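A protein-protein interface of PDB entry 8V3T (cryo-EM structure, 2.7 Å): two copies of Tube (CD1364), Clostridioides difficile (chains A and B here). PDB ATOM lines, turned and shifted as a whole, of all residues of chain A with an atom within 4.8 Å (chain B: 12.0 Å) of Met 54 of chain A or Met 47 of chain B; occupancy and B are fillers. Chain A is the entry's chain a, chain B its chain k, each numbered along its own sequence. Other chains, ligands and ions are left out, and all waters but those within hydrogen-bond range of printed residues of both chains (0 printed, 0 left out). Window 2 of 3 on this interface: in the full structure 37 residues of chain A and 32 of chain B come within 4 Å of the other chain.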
ATOM      1  N   THR A  37      -9.862  -6.305  32.292  1.00  0.00           N
ATOM      2  CA  THR A  37      -9.519  -4.892  32.187  1.00  0.00           C
ATOM      3  C   THR A  37     -10.790  -4.060  32.318  1.00  0.00           C
ATOM      4  O   THR A  37     -11.747  -4.260  31.563  1.00  0.00           O
ATOM      5  CB  THR A  37      -8.823  -4.602  30.858  1.00  0.00           C
ATOM      6  OG1 THR A  37      -7.617  -5.371  30.768  1.00  0.00           O
ATOM      7  CG2 THR A  37      -8.480  -3.129  30.746  1.00  0.00           C
ATOM      8  N   GLU A  39     -12.613  -0.038  33.134  1.00  0.00           N
ATOM      9  CA  GLU A  39     -12.469   1.410  33.055  1.00  0.00           C
ATOM     10  C   GLU A  39     -13.544   2.073  33.903  1.00  0.00           C
ATOM     11  O   GLU A  39     -14.722   1.716  33.809  1.00  0.00           O
ATOM     12  CB  GLU A  39     -12.568   1.893  31.607  1.00  0.00           C
ATOM     13  CG  GLU A  39     -11.443   1.406  30.719  1.00  0.00           C
ATOM     14  CD  GLU A  39     -10.146   2.142  30.978  1.00  0.00           C
ATOM     15  OE1 GLU A  39     -10.200   3.352  31.284  1.00  0.00           O
ATOM     16  OE2 GLU A  39      -9.073   1.511  30.880  1.00  0.00           O
ATOM     17  N   LYS A  52     -16.715  -0.301  33.083  1.00  0.00           N
ATOM     18  CA  LYS A  52     -16.955  -0.868  31.764  1.00  0.00           C
ATOM     19  C   LYS A  52     -15.906  -1.934  31.482  1.00  0.00           C
ATOM     20  O   LYS A  52     -14.707  -1.687  31.645  1.00  0.00           O
ATOM     21  CB  LYS A  52     -16.925   0.217  30.686  1.00  0.00           C
ATOM     22  CG  LYS A  52     -16.680  -0.299  29.283  1.00  0.00           C
ATOM     23  CD  LYS A  52     -17.950  -0.845  28.663  1.00  0.00           C
ATOM     24  CE  LYS A  52     -17.712  -1.272  27.228  1.00  0.00           C
ATOM     25  NZ  LYS A  52     -18.893  -1.950  26.637  1.00  0.00           N
ATOM     26  N   TYR A  53     -16.360  -3.114  31.067  1.00  0.00           N
ATOM     27  CA  TYR A  53     -15.466  -4.228  30.776  1.00  0.00           C
ATOM     28  C   TYR A  53     -14.872  -4.079  29.380  1.00  0.00           C
ATOM     29  O   TYR A  53     -15.598  -3.823  28.414  1.00  0.00           O
ATOM     30  CB  TYR A  53     -16.227  -5.547  30.905  1.00  0.00           C
ATOM     31  CG  TYR A  53     -15.559  -6.742  30.269  1.00  0.00           C
ATOM     32  CD1 TYR A  53     -14.531  -7.413  30.915  1.00  0.00           C
ATOM     33  CD2 TYR A  53     -15.971  -7.214  29.031  1.00  0.00           C
ATOM     34  CE1 TYR A  53     -13.924  -8.512  30.341  1.00  0.00           C
ATOM     35  CE2 TYR A  53     -15.370  -8.311  28.448  1.00  0.00           C
ATOM     36  CZ  TYR A  53     -14.347  -8.955  29.109  1.00  0.00           C
ATOM     37  OH  TYR A  53     -13.747 -10.049  28.533  1.00  0.00           O
ATOM     38  N   MET A  54     -13.549  -4.245  29.271  1.00  0.00           N
ATOM     39  CA  MET A  54     -12.848  -4.026  28.013  1.00  0.00           C
ATOM     40  C   MET A  54     -12.125  -5.247  27.450  1.00  0.00           C
ATOM     41  O   MET A  54     -11.954  -5.320  26.230  1.00  0.00           O
ATOM     42  CB  MET A  54     -11.832  -2.881  28.160  1.00  0.00           C
ATOM     43  CG  MET A  54     -12.399  -1.630  28.811  1.00  0.00           C
ATOM     44  SD  MET A  54     -13.266  -0.545  27.659  1.00  0.00           S
ATOM     45  CE  MET A  54     -12.218  -0.661  26.218  1.00  0.00           C
ATOM     46  N   GLY A  55     -11.710  -6.195  28.281  1.00  0.00           N
ATOM     47  CA  GLY A  55     -10.951  -7.337  27.809  1.00  0.00           C
ATOM     48  C   GLY A  55     -10.330  -8.074  28.981  1.00  0.00           C
ATOM     49  O   GLY A  55     -10.675  -7.831  30.136  1.00  0.00           O
ATOM     50  N   TYR A  56      -9.405  -8.983  28.663  1.00  0.00           N
ATOM     51  CA  TYR A  56      -8.811  -9.788  29.724  1.00  0.00           C
ATOM     52  C   TYR A  56      -7.376 -10.203  29.404  1.00  0.00           C
ATOM     53  O   TYR A  56      -6.934 -10.198  28.252  1.00  0.00           O
ATOM     54  CB  TYR A  56      -9.670 -11.025  30.034  1.00  0.00           C
ATOM     55  CG  TYR A  56      -9.697 -12.089  28.959  1.00  0.00           C
ATOM     56  CD1 TYR A  56      -8.708 -13.058  28.893  1.00  0.00           C
ATOM     57  CD2 TYR A  56     -10.725 -12.140  28.029  1.00  0.00           C
ATOM     58  CE1 TYR A  56      -8.728 -14.034  27.923  1.00  0.00           C
ATOM     59  CE2 TYR A  56     -10.755 -13.117  27.055  1.00  0.00           C
ATOM     60  CZ  TYR A  56      -9.755 -14.060  27.006  1.00  0.00           C
ATOM     61  OH  TYR A  56      -9.788 -15.031  26.034  1.00  0.00           O
ATOM     62  N   ASP B  40       2.631  -6.067  24.513  1.00  0.00           N
ATOM     63  CA  ASP B  40       1.204  -6.331  24.398  1.00  0.00           C
ATOM     64  C   ASP B  40       0.666  -5.830  23.066  1.00  0.00           C
ATOM     65  O   ASP B  40       0.982  -4.722  22.625  1.00  0.00           O
ATOM     66  CB  ASP B  40       0.443  -5.672  25.546  1.00  0.00           C
ATOM     67  CG  ASP B  40       0.556  -6.450  26.835  1.00  0.00           C
ATOM     68  OD1 ASP B  40       1.123  -7.561  26.809  1.00  0.00           O
ATOM     69  OD2 ASP B  40       0.071  -5.956  27.875  1.00  0.00           O
ATOM     70  N   ILE B  41      -0.153  -6.657  22.422  1.00  0.00           N
ATOM     71  CA  ILE B  41      -0.746  -6.333  21.131  1.00  0.00           C
ATOM     72  C   ILE B  41      -2.237  -6.627  21.204  1.00  0.00           C
ATOM     73  O   ILE B  41      -2.637  -7.788  21.342  1.00  0.00           O
ATOM     74  CB  ILE B  41      -0.090  -7.126  19.990  1.00  0.00           C
ATOM     75  CG1 ILE B  41       1.397  -6.781  19.897  1.00  0.00           C
ATOM     76  CG2 ILE B  41      -0.796  -6.847  18.674  1.00  0.00           C
ATOM     77  CD1 ILE B  41       2.044  -7.184  18.603  1.00  0.00           C
ATOM     78  N   ILE B  42      -3.056  -5.586  21.079  1.00  0.00           N
ATOM     79  CA  ILE B  42      -4.508  -5.715  21.081  1.00  0.00           C
ATOM     80  C   ILE B  42      -4.963  -5.882  19.640  1.00  0.00           C
ATOM     81  O   ILE B  42      -4.661  -5.043  18.784  1.00  0.00           O
ATOM     82  CB  ILE B  42      -5.186  -4.500  21.731  1.00  0.00           C
ATOM     83  CG1 ILE B  42      -4.776  -4.369  23.197  1.00  0.00           C
ATOM     84  CG2 ILE B  42      -6.700  -4.597  21.607  1.00  0.00           C
ATOM     85  CD1 ILE B  42      -5.228  -3.085  23.843  1.00  0.00           C
ATOM     86  N   ILE B  43      -5.686  -6.963  19.369  1.00  0.00           N
ATOM     87  CA  ILE B  43      -6.178  -7.279  18.035  1.00  0.00           C
ATOM     88  C   ILE B  43      -7.674  -7.007  18.002  1.00  0.00           C
ATOM     89  O   ILE B  43      -8.408  -7.427  18.904  1.00  0.00           O
ATOM     90  CB  ILE B  43      -5.868  -8.736  17.653  1.00  0.00           C
ATOM     91  CG1 ILE B  43      -4.363  -9.000  17.755  1.00  0.00           C
ATOM     92  CG2 ILE B  43      -6.376  -9.041  16.257  1.00  0.00           C
ATOM     93  CD1 ILE B  43      -3.959 -10.396  17.355  1.00  0.00           C
ATOM     94  N   ALA B  44      -8.120  -6.295  16.970  1.00  0.00           N
ATOM     95  CA  ALA B  44      -9.525  -5.931  16.849  1.00  0.00           C
ATOM     96  C   ALA B  44     -10.405  -7.171  16.766  1.00  0.00           C
ATOM     97  O   ALA B  44     -10.092  -8.124  16.048  1.00  0.00           O
ATOM     98  CB  ALA B  44      -9.735  -5.052  15.618  1.00  0.00           C
ATOM     99  N   GLY B  45     -11.505  -7.156  17.513  1.00  0.00           N
ATOM    100  CA  GLY B  45     -12.444  -8.256  17.500  1.00  0.00           C
ATOM    101  C   GLY B  45     -12.086  -9.423  18.390  1.00  0.00           C
ATOM    102  O   GLY B  45     -12.768 -10.452  18.331  1.00  0.00           O
ATOM    103  N   GLN B  46     -11.047  -9.300  19.212  1.00  0.00           N
ATOM    104  CA  GLN B  46     -10.596 -10.375  20.086  1.00  0.00           C
ATOM    105  C   GLN B  46     -10.499  -9.850  21.511  1.00  0.00           C
ATOM    106  O   GLN B  46      -9.864  -8.821  21.755  1.00  0.00           O
ATOM    107  CB  GLN B  46      -9.243 -10.924  19.617  1.00  0.00           C
ATOM    108  CG  GLN B  46      -8.573 -11.861  20.598  1.00  0.00           C
ATOM    109  CD  GLN B  46      -7.313 -12.490  20.039  1.00  0.00           C
ATOM    110  OE1 GLN B  46      -7.307 -13.015  18.926  1.00  0.00           O
ATOM    111  NE2 GLN B  46      -6.236 -12.442  20.813  1.00  0.00           N
ATOM    112  N   MET B  47     -11.136 -10.555  22.448  1.00  0.00           N
ATOM    113  CA  MET B  47     -11.153 -10.120  23.843  1.00  0.00           C
ATOM    114  C   MET B  47      -9.843 -10.411  24.565  1.00  0.00           C
ATOM    115  O   MET B  47      -9.462  -9.656  25.465  1.00  0.00           O
ATOM    116  CB  MET B  47     -12.322 -10.782  24.577  1.00  0.00           C
ATOM    117  CG  MET B  47     -13.651 -10.008  24.583  1.00  0.00           C
ATOM    118  SD  MET B  47     -13.559  -8.203  24.691  1.00  0.00           S
ATOM    119  CE  MET B  47     -13.483  -7.710  22.973  1.00  0.00           C
ATOM    120  N   GLY B  48      -9.151 -11.490  24.205  1.00  0.00           N
ATOM    121  CA  GLY B  48      -7.901 -11.838  24.852  1.00  0.00           C
ATOM    122  C   GLY B  48      -6.723 -11.211  24.134  1.00  0.00           C
ATOM    123  O   GLY B  48      -6.480 -11.494  22.958  1.00  0.00           O
ATOM    124  N   THR B  49      -5.995 -10.355  24.847  1.00  0.00           N
ATOM    125  CA  THR B  49      -4.858  -9.664  24.255  1.00  0.00           C
ATOM    126  C   THR B  49      -3.664 -10.601  24.127  1.00  0.00           C
ATOM    127  O   THR B  49      -3.439 -11.466  24.974  1.00  0.00           O
ATOM    128  CB  THR B  49      -4.502  -8.437  25.092  1.00  0.00           C
ATOM    129  OG1 THR B  49      -5.699  -7.741  25.476  1.00  0.00           O
ATOM    130  CG2 THR B  49      -3.587  -7.494  24.337  1.00  0.00           C
ATOM    131  N   ASP B  50      -2.902 -10.427  23.055  1.00  0.00           N
ATOM    132  CA  ASP B  50      -1.765 -11.277  22.736  1.00  0.00           C
ATOM    133  C   ASP B  50      -0.461 -10.515  22.943  1.00  0.00           C
ATOM    134  O   ASP B  50      -0.446  -9.325  23.263  1.00  0.00           O
ATOM    135  CB  ASP B  50      -1.857 -11.797  21.294  1.00  0.00           C
ATOM    136  CG  ASP B  50      -1.238 -13.168  21.128  1.00  0.00           C
ATOM    137  OD1 ASP B  50      -0.543 -13.622  22.060  1.00  0.00           O
ATOM    138  OD2 ASP B  50      -1.442 -13.796  20.070  1.00  0.00           O
ATOM    139  N   THR B  51       0.647 -11.231  22.769  1.00  0.00           N
ATOM    140  CA  THR B  51       1.976 -10.706  23.041  1.00  0.00           C
ATOM    141  C   THR B  51       2.909 -11.023  21.884  1.00  0.00           C
ATOM    142  O   THR B  51       2.706 -11.993  21.150  1.00  0.00           O
ATOM    143  CB  THR B  51       2.557 -11.288  24.338  1.00  0.00           C
ATOM    144  OG1 THR B  51       2.534 -12.720  24.272  1.00  0.00           O
ATOM    145  CG2 THR B  51       1.749 -10.831  25.541  1.00  0.00           C
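N of Tyr 56 of chain A sits at hydrogen-bond distance from O of Met 47 of chain B (3.3 Å). O of Met 54 of chain A lies close to SD of Met 47 of chain B (3.6 Å).
No position is printed for both chains.
Among the printed residues, pairs that only touch across the chains: Tyr 53 of chain A with Met 47 of chain B (3.95 Å), Gly 55 of chain A with Met 47 of chain B (3.6 Å), Tyr 56 of chain A with Gly 48 of chain B (3.6 Å) and Tyr 56 of chain A with Thr 49 of chain B (3.5 Å).
The backbone carbonyl oxygen of Thr 37 of chain A lies within hydrogen-bond range of the backbone NH of Met 54 of chain A (2.9 Å). The backbone carbonyl oxygen (O) of Gly 55 of chain A sits at hydrogen-bond distance from the backbone NH (N) of Thr 37 of chain A (2.8 Å).
Met 54 of chain A touches just one residue of chain B: Met 47 (3.6 Å). Of chain A, only Tyr 53 (3.95 Å), Met 54 (3.6 Å), Gly 55 (3.6 Å) and Tyr 56 (3.3 Å) come within 4 Å of Met 47 of chain B. No residue of chain B comes within 4 Å of Thr 37 of chain A. Glu 39 of chain A touches none of the printed residues of chain B. Printed residues of chain B within 4 Å of Tyr 53 of chain A: Met 47. Of chain B, only Met 47 comes within 4 Å of Gly 55 of chain A. Of the printed residues of chain B, Tyr 56 of chain A touches Met 47, Gly 48 and Thr 49. Printed residues of chain A within 4 Å of Thr 49 of chain B: Tyr 56. Of the printed residues of chain A, Gly 48 of chain B touches Tyr 56 (3.6 Å). Thr 51 of chain B touches none of the printed residues of chain A. The nearest residue of chain B that does not touch Met 54 of chain A is Gln 46 of chain B (6.1 Å). The nearest printed residue of chain A that does not touch Met 47 of chain B is Thr 37 of chain A (7.1 Å).
Hydrophobic or aromatic side chains of chain A within 4 Å of the printed part of chain B: Tyr 53 and Tyr 56. Printed residues of chain B that touch a printed residue of chain A: Met 47, Gly 48 and Thr 49. Hydrophobic or aromatic side chains of chain B that line the printed part of chain A: Met 47. Among the printed residues, 6 pairs touch across the chains. Among the printed residues, no Asp or Glu carboxylate lies within 4 Å of a Lys or Arg side-chain nitrogen of the other chain.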
